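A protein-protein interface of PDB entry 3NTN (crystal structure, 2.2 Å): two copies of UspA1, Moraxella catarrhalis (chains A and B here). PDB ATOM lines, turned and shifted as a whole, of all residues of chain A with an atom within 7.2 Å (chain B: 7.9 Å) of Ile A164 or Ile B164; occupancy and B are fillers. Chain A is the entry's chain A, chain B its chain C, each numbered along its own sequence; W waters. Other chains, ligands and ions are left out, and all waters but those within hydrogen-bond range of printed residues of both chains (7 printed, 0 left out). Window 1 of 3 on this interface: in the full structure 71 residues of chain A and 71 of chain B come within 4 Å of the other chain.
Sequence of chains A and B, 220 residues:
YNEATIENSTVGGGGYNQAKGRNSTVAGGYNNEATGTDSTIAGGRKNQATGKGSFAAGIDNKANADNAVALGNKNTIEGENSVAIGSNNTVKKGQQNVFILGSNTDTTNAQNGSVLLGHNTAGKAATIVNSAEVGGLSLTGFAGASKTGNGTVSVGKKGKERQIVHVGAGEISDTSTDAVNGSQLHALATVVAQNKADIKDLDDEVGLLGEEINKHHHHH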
ATOM      1  N   VAL A 153       9.268  -1.787  -1.206  1.00  0.00           N
ATOM      2  CA  VAL A 153      10.200  -1.257  -2.153  1.00  0.00           C
ATOM      3  C   VAL A 153      10.181  -2.133  -3.378  1.00  0.00           C
ATOM      4  O   VAL A 153      10.384  -3.343  -3.273  1.00  0.00           O
ATOM      5  CB  VAL A 153      11.613  -1.224  -1.537  1.00  0.00           C
ATOM      6  CG1 VAL A 153      12.627  -0.719  -2.565  1.00  0.00           C
ATOM      7  CG2 VAL A 153      11.601  -0.295  -0.318  1.00  0.00           C
ATOM      8  N   SER A 154       9.922  -1.572  -4.558  1.00  0.00           N
ATOM      9  CA  SER A 154       9.843  -2.452  -5.751  1.00  0.00           C
ATOM     10  C   SER A 154      10.966  -2.182  -6.665  1.00  0.00           C
ATOM     11  O   SER A 154      11.365  -1.003  -6.838  1.00  0.00           O
ATOM     12  CB  SER A 154       8.541  -2.233  -6.517  1.00  0.00           C
ATOM     13  OG  SER A 154       8.495  -3.104  -7.646  1.00  0.00           O
ATOM     14  N   VAL A 155      11.537  -3.257  -7.213  1.00  0.00           N
ATOM     15  CA  VAL A 155      12.604  -3.115  -8.202  1.00  0.00           C
ATOM     16  C   VAL A 155      12.207  -3.533  -9.603  1.00  0.00           C
ATOM     17  O   VAL A 155      13.036  -3.477 -10.519  1.00  0.00           O
ATOM     18  CB  VAL A 155      13.905  -3.844  -7.797  1.00  0.00           C
ATOM     19  CG1 VAL A 155      14.408  -3.337  -6.466  1.00  0.00           C
ATOM     20  CG2 VAL A 155      13.753  -5.408  -7.793  1.00  0.00           C
ATOM     21  N   ARG A 162      13.970  -7.735 -11.474  1.00  0.00           N
ATOM     22  CA  ARG A 162      15.356  -7.319 -11.561  1.00  0.00           C
ATOM     23  C   ARG A 162      16.167  -7.962 -10.440  1.00  0.00           C
ATOM     24  O   ARG A 162      15.788  -7.895  -9.256  1.00  0.00           O
ATOM     25  CB  ARG A 162      15.503  -5.802 -11.459  1.00  0.00           C
ATOM     26  CG  ARG A 162      15.266  -5.026 -12.699  1.00  0.00           C
ATOM     27  CD  ARG A 162      15.564  -3.508 -12.552  1.00  0.00           C
ATOM     28  NE  ARG A 162      15.159  -2.878 -13.811  1.00  0.00           N
ATOM     29  CZ  ARG A 162      13.997  -2.288 -14.092  1.00  0.00           C
ATOM     30  NH1 ARG A 162      13.051  -2.093 -13.183  1.00  0.00           N
ATOM     31  NH2 ARG A 162      13.818  -1.824 -15.311  1.00  0.00           N
ATOM     32  N   GLN A 163      17.292  -8.566 -10.825  1.00  0.00           N
ATOM     33  CA  GLN A 163      18.288  -8.964  -9.867  1.00  0.00           C
ATOM     34  C   GLN A 163      18.818  -7.765  -9.089  1.00  0.00           C
ATOM     35  O   GLN A 163      18.960  -6.674  -9.642  1.00  0.00           O
ATOM     36  CB  GLN A 163      19.414  -9.657 -10.611  1.00  0.00           C
ATOM     37  CG  GLN A 163      19.053 -11.038 -11.090  1.00  0.00           C
ATOM     38  CD  GLN A 163      20.148 -11.672 -11.928  1.00  0.00           C
ATOM     39  OE1 GLN A 163      20.768 -11.006 -12.778  1.00  0.00           O
ATOM     40  NE2 GLN A 163      20.379 -12.968 -11.708  1.00  0.00           N
ATOM     41  N   ILE A 164      19.086  -7.963  -7.795  1.00  0.00           N
ATOM     42  CA  ILE A 164      19.818  -6.959  -6.982  1.00  0.00           C
ATOM     43  C   ILE A 164      21.265  -7.441  -6.828  1.00  0.00           C
ATOM     44  O   ILE A 164      21.483  -8.626  -6.493  1.00  0.00           O
ATOM     45  CB  ILE A 164      19.152  -6.627  -5.628  1.00  0.00           C
ATOM     46  CG1 ILE A 164      17.641  -6.449  -5.869  1.00  0.00           C
ATOM     47  CG2 ILE A 164      19.817  -5.351  -5.056  1.00  0.00           C
ATOM     48  CD1 ILE A 164      16.739  -5.904  -4.727  1.00  0.00           C
ATOM     49  N   VAL A 165      22.236  -6.579  -7.119  1.00  0.00           N
ATOM     50  CA  VAL A 165      23.617  -7.046  -7.244  1.00  0.00           C
ATOM     51  C   VAL A 165      24.574  -6.268  -6.340  1.00  0.00           C
ATOM     52  O   VAL A 165      24.244  -5.127  -5.924  1.00  0.00           O
ATOM     53  CB  VAL A 165      24.140  -7.037  -8.715  1.00  0.00           C
ATOM     54  CG1 VAL A 165      23.279  -8.004  -9.653  1.00  0.00           C
ATOM     55  CG2 VAL A 165      24.241  -5.645  -9.253  1.00  0.00           C
ATOM     56  N   HIS A 166      25.721  -6.896  -6.031  1.00  0.00           N
ATOM     57  CA  HIS A 166      26.717  -6.330  -5.113  1.00  0.00           C
ATOM     58  C   HIS A 166      26.168  -6.102  -3.708  1.00  0.00           C
ATOM     59  O   HIS A 166      26.480  -5.078  -3.066  1.00  0.00           O
ATOM     60  CB  HIS A 166      27.300  -5.055  -5.687  1.00  0.00           C
ATOM     61  CG  HIS A 166      28.012  -5.275  -6.972  1.00  0.00           C
ATOM     62  ND1 HIS A 166      29.017  -6.214  -7.108  1.00  0.00           N
ATOM     63  CD2 HIS A 166      27.834  -4.726  -8.193  1.00  0.00           C
ATOM     64  CE1 HIS A 166      29.422  -6.233  -8.365  1.00  0.00           C
ATOM     65  NE2 HIS A 166      28.733  -5.332  -9.041  1.00  0.00           N
ATOM     66  N   VAL A 167      25.336  -7.044  -3.258  1.00  0.00           N
ATOM     67  CA  VAL A 167      24.711  -7.080  -1.924  1.00  0.00           C
ATOM     68  C   VAL A 167      25.669  -7.728  -0.914  1.00  0.00           C
ATOM     69  O   VAL A 167      26.113  -8.881  -1.098  1.00  0.00           O
ATOM     70  CB  VAL A 167      23.390  -7.917  -2.001  1.00  0.00           C
ATOM     71  CG1 VAL A 167      22.694  -8.031  -0.629  1.00  0.00           C
ATOM     72  CG2 VAL A 167      22.453  -7.268  -3.054  1.00  0.00           C
ATOM     73  N   GLY A 168      26.008  -6.990   0.140  1.00  0.00           N
ATOM     74  CA  GLY A 168      26.829  -7.525   1.222  1.00  0.00           C
ATOM     75  C   GLY A 168      26.147  -8.653   1.971  1.00  0.00           C
ATOM     76  O   GLY A 168      24.893  -8.708   2.053  1.00  0.00           O
ATOM     77  N   ALA A 169      26.970  -9.561   2.503  1.00  0.00           N
ATOM     78  CA  ALA A 169      26.472 -10.688   3.316  1.00  0.00           C
ATOM     79  C   ALA A 169      25.671 -10.164   4.484  1.00  0.00           C
ATOM     80  O   ALA A 169      26.105  -9.303   5.226  1.00  0.00           O
ATOM     81  CB  ALA A 169      27.604 -11.530   3.802  1.00  0.00           C
ATOM     82  N   GLY A 170      24.448 -10.679   4.614  1.00  0.00           N
ATOM     83  CA  GLY A 170      23.557 -10.328   5.737  1.00  0.00           C
ATOM     84  C   GLY A 170      23.847 -11.095   7.003  1.00  0.00           C
ATOM     85  O   GLY A 170      24.301 -12.243   6.975  1.00  0.00           O
ATOM     86  N   THR A 177      17.257  -8.844   9.873  1.00  0.00           N
ATOM     87  CA  THR A 177      16.407  -8.299   8.849  1.00  0.00           C
ATOM     88  C   THR A 177      17.280  -7.807   7.704  1.00  0.00           C
ATOM     89  O   THR A 177      16.863  -6.965   6.910  1.00  0.00           O
ATOM     90  CB  THR A 177      15.528  -7.209   9.441  1.00  0.00           C
ATOM     91  OG1 THR A 177      14.651  -6.733   8.426  1.00  0.00           O
ATOM     92  CG2 THR A 177      16.348  -6.068   9.952  1.00  0.00           C
ATOM     93  N   ASP A 178      18.497  -8.355   7.613  1.00  0.00           N
ATOM     94  CA  ASP A 178      19.424  -7.947   6.551  1.00  0.00           C
ATOM     95  C   ASP A 178      19.029  -8.810   5.336  1.00  0.00           C
ATOM     96  O   ASP A 178      18.595  -9.922   5.513  1.00  0.00           O
ATOM     97  CB  ASP A 178      20.897  -8.267   6.874  1.00  0.00           C
ATOM     98  CG  ASP A 178      21.481  -7.484   8.067  1.00  0.00           C
ATOM     99  OD1 ASP A 178      22.625  -7.885   8.431  1.00  0.00           O
ATOM    100  OD2 ASP A 178      20.855  -6.532   8.656  1.00  0.00           O
ATOM    101  N   ALA A 179      19.174  -8.297   4.124  1.00  0.00           N
ATOM    102  CA  ALA A 179      19.062  -9.135   2.940  1.00  0.00           C
ATOM    103  C   ALA A 179      20.131 -10.207   2.953  1.00  0.00           C
ATOM    104  O   ALA A 179      21.232 -10.014   3.444  1.00  0.00           O
ATOM    105  CB  ALA A 179      19.149  -8.298   1.659  1.00  0.00           C
ATOM    106  N   VAL A 180      19.779 -11.362   2.408  1.00  0.00           N
ATOM    107  CA  VAL A 180      20.702 -12.495   2.167  1.00  0.00           C
ATOM    108  C   VAL A 180      21.208 -12.523   0.685  1.00  0.00           C
ATOM    109  O   VAL A 180      20.446 -12.236  -0.240  1.00  0.00           O
ATOM    110  CB  VAL A 180      19.945 -13.788   2.558  1.00  0.00           C
ATOM    111  CG1 VAL A 180      20.608 -15.008   2.048  1.00  0.00           C
ATOM    112  CG2 VAL A 180      19.778 -13.842   4.149  1.00  0.00           C
ATOM    113  N   ASN A 181      22.474 -12.892   0.476  1.00  0.00           N
ATOM    114  CA  ASN A 181      23.034 -13.009  -0.877  1.00  0.00           C
ATOM    115  C   ASN A 181      23.248 -14.465  -1.292  1.00  0.00           C
ATOM    116  O   ASN A 181      23.203 -15.329  -0.442  1.00  0.00           O
ATOM    117  CB  ASN A 181      24.252 -12.093  -1.122  1.00  0.00           C
ATOM    118  CG  ASN A 181      25.520 -12.541  -0.447  1.00  0.00           C
ATOM    119  OD1 ASN A 181      25.691 -13.697  -0.145  1.00  0.00           O
ATOM    120  ND2 ASN A 181      26.493 -11.629  -0.334  1.00  0.00           N
ATOM    121  N   VAL B 115      19.383   0.281 -12.419  1.00  0.00           N
ATOM    122  CA  VAL B 115      19.382   1.306 -11.365  1.00  0.00           C
ATOM    123  C   VAL B 115      20.677   1.165 -10.532  1.00  0.00           C
ATOM    124  O   VAL B 115      21.003   0.074 -10.083  1.00  0.00           O
ATOM    125  CB  VAL B 115      18.103   1.198 -10.418  1.00  0.00           C
ATOM    126  CG1 VAL B 115      18.066   2.303  -9.350  1.00  0.00           C
ATOM    127  CG2 VAL B 115      16.825   1.266 -11.228  1.00  0.00           C
ATOM    128  N   LEU B 117      22.635   2.611  -7.077  1.00  0.00           N
ATOM    129  CA  LEU B 117      22.501   3.374  -5.854  1.00  0.00           C
ATOM    130  C   LEU B 117      23.824   3.493  -5.104  1.00  0.00           C
ATOM    131  O   LEU B 117      24.519   2.498  -4.890  1.00  0.00           O
ATOM    132  CB  LEU B 117      21.432   2.782  -4.930  1.00  0.00           C
ATOM    133  CG  LEU B 117      20.010   2.543  -5.502  1.00  0.00           C
ATOM    134  CD1 LEU B 117      19.232   1.762  -4.503  1.00  0.00           C
ATOM    135  CD2 LEU B 117      19.278   3.892  -5.787  1.00  0.00           C
ATOM    136  N   LYS B 124      25.858  -3.833 -13.663  1.00  0.00           N
ATOM    137  CA  LYS B 124      26.130  -5.252 -13.921  1.00  0.00           C
ATOM    138  C   LYS B 124      25.031  -5.835 -14.828  1.00  0.00           C
ATOM    139  O   LYS B 124      23.842  -5.534 -14.658  1.00  0.00           O
ATOM    140  CB  LYS B 124      26.167  -5.990 -12.577  1.00  0.00           C
ATOM    141  CG  LYS B 124      27.087  -7.198 -12.566  1.00  0.00           C
ATOM    142  CD  LYS B 124      27.086  -7.824 -11.200  1.00  0.00           C
ATOM    143  CE  LYS B 124      27.169  -9.340 -11.259  1.00  0.00           C
ATOM    144  NZ  LYS B 124      27.844  -9.768 -10.023  1.00  0.00           N
ATOM    145  N   GLY B 151      18.013  -5.315 -17.132  1.00  0.00           N
ATOM    146  CA  GLY B 151      18.840  -4.479 -16.277  1.00  0.00           C
ATOM    147  C   GLY B 151      18.906  -5.022 -14.870  1.00  0.00           C
ATOM    148  O   GLY B 151      18.241  -5.989 -14.555  1.00  0.00           O
ATOM    149  N   THR B 152      19.724  -4.414 -14.020  1.00  0.00           N
ATOM    150  CA  THR B 152      19.815  -4.840 -12.631  1.00  0.00           C
ATOM    151  C   THR B 152      19.744  -3.653 -11.736  1.00  0.00           C
ATOM    152  O   THR B 152      19.902  -2.551 -12.184  1.00  0.00           O
ATOM    153  CB  THR B 152      21.124  -5.591 -12.311  1.00  0.00           C
ATOM    154  OG1 THR B 152      22.233  -4.856 -12.814  1.00  0.00           O
ATOM    155  CG2 THR B 152      21.114  -6.984 -12.890  1.00  0.00           C
ATOM    156  N   VAL B 153      19.488  -3.882 -10.463  1.00  0.00           N
ATOM    157  CA  VAL B 153      19.532  -2.836  -9.471  1.00  0.00           C
ATOM    158  C   VAL B 153      20.798  -3.054  -8.681  1.00  0.00           C
ATOM    159  O   VAL B 153      20.978  -4.091  -8.081  1.00  0.00           O
ATOM    160  CB  VAL B 153      18.304  -2.864  -8.556  1.00  0.00           C
ATOM    161  CG1 VAL B 153      18.424  -1.833  -7.442  1.00  0.00           C
ATOM    162  CG2 VAL B 153      17.074  -2.631  -9.356  1.00  0.00           C
ATOM    163  N   SER B 154      21.692  -2.071  -8.698  1.00  0.00           N
ATOM    164  CA  SER B 154      23.045  -2.267  -8.036  1.00  0.00           C
ATOM    165  C   SER B 154      23.217  -1.436  -6.830  1.00  0.00           C
ATOM    166  O   SER B 154      22.777  -0.271  -6.782  1.00  0.00           O
ATOM    167  CB  SER B 154      24.202  -2.002  -8.970  1.00  0.00           C
ATOM    168  OG  SER B 154      25.441  -2.282  -8.313  1.00  0.00           O
ATOM    169  N   VAL B 155      23.758  -2.072  -5.799  1.00  0.00           N
ATOM    170  CA  VAL B 155      24.018  -1.347  -4.549  1.00  0.00           C
ATOM    171  C   VAL B 155      25.483  -1.190  -4.209  1.00  0.00           C
ATOM    172  O   VAL B 155      25.794  -0.673  -3.139  1.00  0.00           O
ATOM    173  CB  VAL B 155      23.281  -1.972  -3.352  1.00  0.00           C
ATOM    174  CG1 VAL B 155      21.807  -2.000  -3.628  1.00  0.00           C
ATOM    175  CG2 VAL B 155      23.761  -3.377  -3.041  1.00  0.00           C
ATOM    176  N   GLY B 156      26.412  -1.602  -5.078  1.00  0.00           N
ATOM    177  CA  GLY B 156      27.842  -1.468  -4.671  1.00  0.00           C
ATOM    178  C   GLY B 156      28.719  -1.832  -5.842  1.00  0.00           C
ATOM    179  O   GLY B 156      28.259  -1.707  -6.955  1.00  0.00           O
ATOM    180  N   GLU B 161      30.797  -4.337  -1.572  1.00  0.00           N
ATOM    181  CA  GLU B 161      29.373  -4.682  -1.510  1.00  0.00           C
ATOM    182  C   GLU B 161      28.713  -3.939  -0.347  1.00  0.00           C
ATOM    183  O   GLU B 161      29.388  -3.522   0.581  1.00  0.00           O
ATOM    184  CB  GLU B 161      29.136  -6.210  -1.429  1.00  0.00           C
ATOM    185  CG  GLU B 161      29.621  -6.987  -2.668  1.00  0.00           C
ATOM    186  CD  GLU B 161      31.141  -7.263  -2.671  1.00  0.00           C
ATOM    187  OE1 GLU B 161      31.620  -7.970  -3.585  1.00  0.00           O
ATOM    188  OE2 GLU B 161      31.878  -6.768  -1.783  1.00  0.00           O
ATOM    189  N   ARG B 162      27.408  -3.731  -0.429  1.00  0.00           N
ATOM    190  CA  ARG B 162      26.666  -3.078   0.649  1.00  0.00           C
ATOM    191  C   ARG B 162      25.576  -4.006   1.132  1.00  0.00           C
ATOM    192  O   ARG B 162      24.798  -4.532   0.305  1.00  0.00           O
ATOM    193  CB  ARG B 162      25.977  -1.792   0.173  1.00  0.00           C
ATOM    194  CG  ARG B 162      26.809  -0.554   0.200  1.00  0.00           C
ATOM    195  CD  ARG B 162      26.073   0.739  -0.269  1.00  0.00           C
ATOM    196  NE  ARG B 162      27.045   1.815  -0.269  1.00  0.00           N
ATOM    197  CZ  ARG B 162      27.713   2.265  -1.330  1.00  0.00           C
ATOM    198  NH1 ARG B 162      27.479   1.824  -2.557  1.00  0.00           N
ATOM    199  NH2 ARG B 162      28.609   3.219  -1.162  1.00  0.00           N
ATOM    200  N   GLN B 163      25.490  -4.151   2.458  1.00  0.00           N
ATOM    201  CA  GLN B 163      24.382  -4.816   3.059  1.00  0.00           C
ATOM    202  C   GLN B 163      23.070  -4.062   2.813  1.00  0.00           C
ATOM    203  O   GLN B 163      23.045  -2.842   2.816  1.00  0.00           O
ATOM    204  CB  GLN B 163      24.646  -4.944   4.517  1.00  0.00           C
ATOM    205  CG  GLN B 163      25.719  -5.952   4.876  1.00  0.00           C
ATOM    206  CD  GLN B 163      25.974  -5.976   6.360  1.00  0.00           C
ATOM    207  OE1 GLN B 163      26.117  -4.920   6.994  1.00  0.00           O
ATOM    208  NE2 GLN B 163      26.051  -7.171   6.928  1.00  0.00           N
ATOM    209  N   ILE B 164      21.988  -4.780   2.551  1.00  0.00           N
ATOM    210  CA  ILE B 164      20.646  -4.134   2.533  1.00  0.00           C
ATOM    211  C   ILE B 164      19.953  -4.373   3.883  1.00  0.00           C
ATOM    212  O   ILE B 164      19.955  -5.487   4.351  1.00  0.00           O
ATOM    213  CB  ILE B 164      19.797  -4.548   1.331  1.00  0.00           C
ATOM    214  CG1 ILE B 164      20.662  -4.435   0.062  1.00  0.00           C
ATOM    215  CG2 ILE B 164      18.558  -3.630   1.261  1.00  0.00           C
ATOM    216  CD1 ILE B 164      19.959  -4.769  -1.288  1.00  0.00           C
ATOM    217  N   VAL B 165      19.416  -3.342   4.531  1.00  0.00           N
ATOM    218  CA  VAL B 165      18.983  -3.513   5.935  1.00  0.00           C
ATOM    219  C   VAL B 165      17.549  -3.082   6.177  1.00  0.00           C
ATOM    220  O   VAL B 165      16.990  -2.327   5.366  1.00  0.00           O
ATOM    221  CB  VAL B 165      19.911  -2.781   6.961  1.00  0.00           C
ATOM    222  CG1 VAL B 165      21.385  -3.349   6.909  1.00  0.00           C
ATOM    223  CG2 VAL B 165      19.864  -1.279   6.756  1.00  0.00           C
ATOM    224  N   HIS B 166      16.934  -3.600   7.244  1.00  0.00           N
ATOM    225  CA  HIS B 166      15.513  -3.373   7.526  1.00  0.00           C
ATOM    226  C   HIS B 166      14.595  -3.856   6.392  1.00  0.00           C
ATOM    227  O   HIS B 166      13.573  -3.183   6.031  1.00  0.00           O
ATOM    228  CB  HIS B 166      15.280  -1.918   7.805  1.00  0.00           C
ATOM    229  CG  HIS B 166      16.035  -1.417   8.978  1.00  0.00           C
ATOM    230  ND1 HIS B 166      15.934  -1.999  10.229  1.00  0.00           N
ATOM    231  CD2 HIS B 166      16.917  -0.404   9.099  1.00  0.00           C
ATOM    232  CE1 HIS B 166      16.746  -1.375  11.061  1.00  0.00           C
ATOM    233  NE2 HIS B 166      17.347  -0.400  10.408  1.00  0.00           N
ATOM    234  N   VAL B 167      14.961  -5.028   5.850  1.00  0.00           N
ATOM    235  CA  VAL B 167      14.196  -5.745   4.867  1.00  0.00           C
ATOM    236  C   VAL B 167      13.111  -6.606   5.578  1.00  0.00           C
ATOM    237  O   VAL B 167      13.427  -7.443   6.466  1.00  0.00           O
ATOM    238  CB  VAL B 167      15.138  -6.642   4.037  1.00  0.00           C
ATOM    239  CG1 VAL B 167      14.373  -7.475   2.970  1.00  0.00           C
ATOM    240  CG2 VAL B 167      16.315  -5.769   3.443  1.00  0.00           C
ATOM    241  N   THR B 177       8.986 -13.694  -5.538  1.00  0.00           N
ATOM    242  CA  THR B 177      10.066 -12.864  -6.008  1.00  0.00           C
ATOM    243  C   THR B 177      10.338 -11.824  -4.960  1.00  0.00           C
ATOM    244  O   THR B 177      10.875 -10.752  -5.255  1.00  0.00           O
ATOM    245  CB  THR B 177       9.706 -12.193  -7.332  1.00  0.00           C
ATOM    246  OG1 THR B 177       8.458 -11.501  -7.177  1.00  0.00           O
ATOM    247  CG2 THR B 177       9.582 -13.237  -8.481  1.00  0.00           C
ATOM    248  N   ALA B 179      12.405 -10.486  -1.781  1.00  0.00           N
ATOM    249  CA  ALA B 179      13.704 -10.737  -1.120  1.00  0.00           C
ATOM    250  C   ALA B 179      13.533 -11.401   0.233  1.00  0.00           C
ATOM    251  O   ALA B 179      12.525 -11.204   0.938  1.00  0.00           O
ATOM    252  CB  ALA B 179      14.506  -9.469  -0.956  1.00  0.00           C
ATOM    253  N   VAL B 180      14.591 -12.117   0.609  1.00  0.00           N
ATOM    254  CA  VAL B 180      14.675 -12.966   1.811  1.00  0.00           C
ATOM    255  C   VAL B 180      15.630 -12.286   2.792  1.00  0.00           C
ATOM    256  O   VAL B 180      16.659 -11.718   2.393  1.00  0.00           O
ATOM    257  CB  VAL B 180      15.143 -14.430   1.353  1.00  0.00           C
ATOM    258  CG1 VAL B 180      15.805 -15.234   2.415  1.00  0.00           C
ATOM    259  CG2 VAL B 180      13.909 -15.181   0.757  1.00  0.00           C
ATOM    260  N   ASN B 181      15.271 -12.290   4.071  1.00  0.00           N
ATOM    261  CA  ASN B 181      16.148 -11.693   5.074  1.00  0.00           C
ATOM    262  C   ASN B 181      16.833 -12.763   5.905  1.00  0.00           C
ATOM    263  O   ASN B 181      16.465 -13.922   5.817  1.00  0.00           O
ATOM    264  CB  ASN B 181      15.420 -10.598   5.902  1.00  0.00           C
ATOM    265  CG  ASN B 181      14.395 -11.126   6.866  1.00  0.00           C
ATOM    266  OD1 ASN B 181      14.442 -12.272   7.241  1.00  0.00           O
ATOM    267  ND2 ASN B 181      13.506 -10.258   7.350  1.00  0.00           N
ATOM    268  N   GLY B 182      17.848 -12.375   6.693  1.00  0.00           N
ATOM    269  CA  GLY B 182      18.655 -13.328   7.450  1.00  0.00           C
ATOM    270  C   GLY B 182      17.909 -14.297   8.367  1.00  0.00           C
ATOM    271  O   GLY B 182      18.342 -15.443   8.574  1.00  0.00           O
HETATM  272  O   HOH W   1      17.640 -11.281  -0.305  1.00  0.00           O
HETATM  273  O   HOH W   2      28.781  -8.290   5.501  1.00  0.00           O
HETATM  274  O   HOH W   3      18.050  -8.678 -13.540  1.00  0.00           O
HETATM  275  O   HOH W   4      22.388  -7.661   3.201  1.00  0.00           O
HETATM  276  O   HOH W   5      30.127  -8.335  -5.707  1.00  0.00           O
HETATM  277  O   HOH W   6      26.361  -9.393  -7.518  1.00  0.00           O
HETATM  278  O   HOH W   7      18.788  -4.965   9.244  1.00  0.00           O
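O of Gln A163 sits at hydrogen-bond distance from N of Val B153, 3.0 Å away.
N of Val B155 lies within hydrogen-bond range of O of Val A165 (3.1 Å).
The backbone carbonyl oxygen (O) of Ala A169 lies within hydrogen-bond range of the side-chain amide nitrogen (NE2) of Gln B163.
The backbone NH (N) of Ala A179 lies within hydrogen-bond range of the backbone carbonyl oxygen (O) of Ile B164, at 2.9 Å.
The backbone carbonyl oxygen (O) of Asp A178 lies within hydrogen-bond range of the backbone NH (N) of Gly B182 (2.8 Å).
N of Gly A168 lies within hydrogen-bond range of O of Arg B162.
The backbone carbonyl oxygen of Val B180 is in hydrogen-bond range of the backbone NH of Val A180 (3.1 Å).
The backbone carbonyl oxygen of Val B167 lies within hydrogen-bond range of the side-chain hydroxyl of Thr A177 (2.4 Å).
N of Val A165 lies within hydrogen-bond range of O of Val B153, 2.9 Å away.
N of His B166 sits at hydrogen-bond distance from O of Thr A177 (3.4 Å).
The backbone carbonyl oxygen (O) of His A166 lies within hydrogen-bond range of the backbone NH (N) of Arg B162, 3.1 Å away.
Of the 21 printed residues of chain B, 17 touch a printed residue of chain A.
Printed residues of chain B that touch a printed residue of chain A: Lys B124, Gly B151, Thr B152, Val B153, Ser B154, Val B155, Gly B156, Glu B161, Arg B162, Gln B163, Ile B164, Val B165, His B166, Val B167, Val B180, Asn B181 and Gly B182.
Along chain B the printed residues that touch a printed residue of chain A span positions 124 to 182.
Of the 17 printed residues of chain A, 13 touch a printed residue of chain B.
Among the printed residues, 39 pairs touch across the chains.
Among the printed residues, no Asp or Glu carboxylate lies within 4 Å of a Lys or Arg side-chain nitrogen of the other chain.
Ile A164 touches just these residues of chain B: Val B153 and Ile B164.
Of the printed residues of chain B, Val A167 touches Val B155, Glu B161, Arg B162 and Ile B164.
Printed residues of chain B within 4 Å of Gly A168: Glu B161 (3.6 Å), Arg B162 (2.7 Å) and Gln B163 (3.7 Å).
Of the printed residues of chain B, Thr A177 touches His B166 (3.4 Å), Val B167 (2.4 Å) and Asn B181 (3.8 Å).
Of the printed residues of chain A, Val B153 touches Val A155 (3.7 Å), Arg A162 (3.6 Å), Gln A163 (3.0 Å), Ile A164 (3.3 Å) and Val A165 (2.9 Å).
Of the printed residues of chain A, Val B155 touches Val A165, His A166 and Val A167.
Of chain A, only Ile A164 (3.8 Å), Val A167 (3.9 Å), Asp A178 (3.3 Å) and Ala A179 (2.9 Å) come within 4 Å of Ile B164.
The nearest residue of chain B that does not touch Ile A164 is Val B155 (4.2 Å).
N of Gly A170 sits close to O of Ala A179 (3.5 Å).
The backbone carbonyl oxygen of Val A155 is in hydrogen-bond range of the guanidinium group of Arg A162 (3.0 Å).
The backbone carbonyl oxygen (O) of Val B115 is in hydrogen-bond range of the backbone NH (N) of Ser B154, 2.6 Å away.
The side-chain amide nitrogen (ND2) of Asn A181 sits at hydrogen-bond distance from the backbone carbonyl oxygen (O) of Val A167, 2.9 Å away.
Gln A163 touches Val B153, but with the chains exchanged Val A153 does not touch Gln B163 (11.9 Å).
Ile A164 touches its own counterpart, Ile B164.
Thr A177 touches Val B167, but with the chains exchanged Val A167 does not touch Thr B177 (12.3 Å).
Ala A179 touches Val B180, but with the chains exchanged Val A180 does not touch Ala B179 (6.5 Å).
Water W5 lies within hydrogen-bond range of OE1 of Glu B161 and ND1 of His A166.
Water W4 lies within hydrogen-bond range of O of Ala A179 (2.6 Å), O of Gly A168 (2.9 Å) and N of Ile B164 (3.0 Å).
Water W3 bridges N of Gln A163 and O of Gly B151.
Water W2 lies within hydrogen-bond range of O of Ala A169 and NE2 of Gln B163.
Water W1 lies within hydrogen-bond range of the backbone carbonyl oxygen (O) of Val B180 (2.9 Å) and the backbone carbonyl oxygen (O) of Val A180 (3.0 Å).
Water W6 bridges NZ of Lys B124 (2.9 Å) and N of His A166 (3.0 Å).
Among the printed residues, merely in contact across the chains: Asp A178 with Asn B181 (3.1 Å), His A166 with Val B155 (3.2 Å), Ile A164 with Val B153 (3.3 Å), His A166 with Gly B156 (3.3 Å), His A166 with Glu B161 (3.3 Å), Asp A178 with Ile B164 (3.3 Å), Val A167 with Arg B162 (3.4 Å), His A166 with Ser B154 (3.4 Å), Val A180 with Gly B182 (3.5 Å), Ala A179 with Val B180 (3.6 Å), Gly A168 with Glu B161 (3.6 Å), Val A180 with Asn B181 (3.6 Å), Gln A163 with Thr B152 (3.6 Å), Arg A162 with Gly B151 (3.6 Å), Arg A162 with Val B153 (3.6 Å), Val A165 with Ser B154 (3.7 Å), Asp A178 with Val B165 (3.7 Å), His A166 with Lys B124 (3.7 Å), Gly A168 with Gln B163 (3.7 Å), Val A155 with Val B153 (3.7 Å), Thr A177 with Asn B181 (3.8 Å), Asp A178 with Gln B163 (3.8 Å), Ile A164 with Ile B164 (3.8 Å), Val A167 with Glu B161 (3.8 Å), Val A165 with Lys B124 (3.9 Å), Ala A179 with Val B167 (3.9 Å), Val A167 with Ile B164 (3.9 Å) and Val A167 with Val B155 (3.98 Å).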
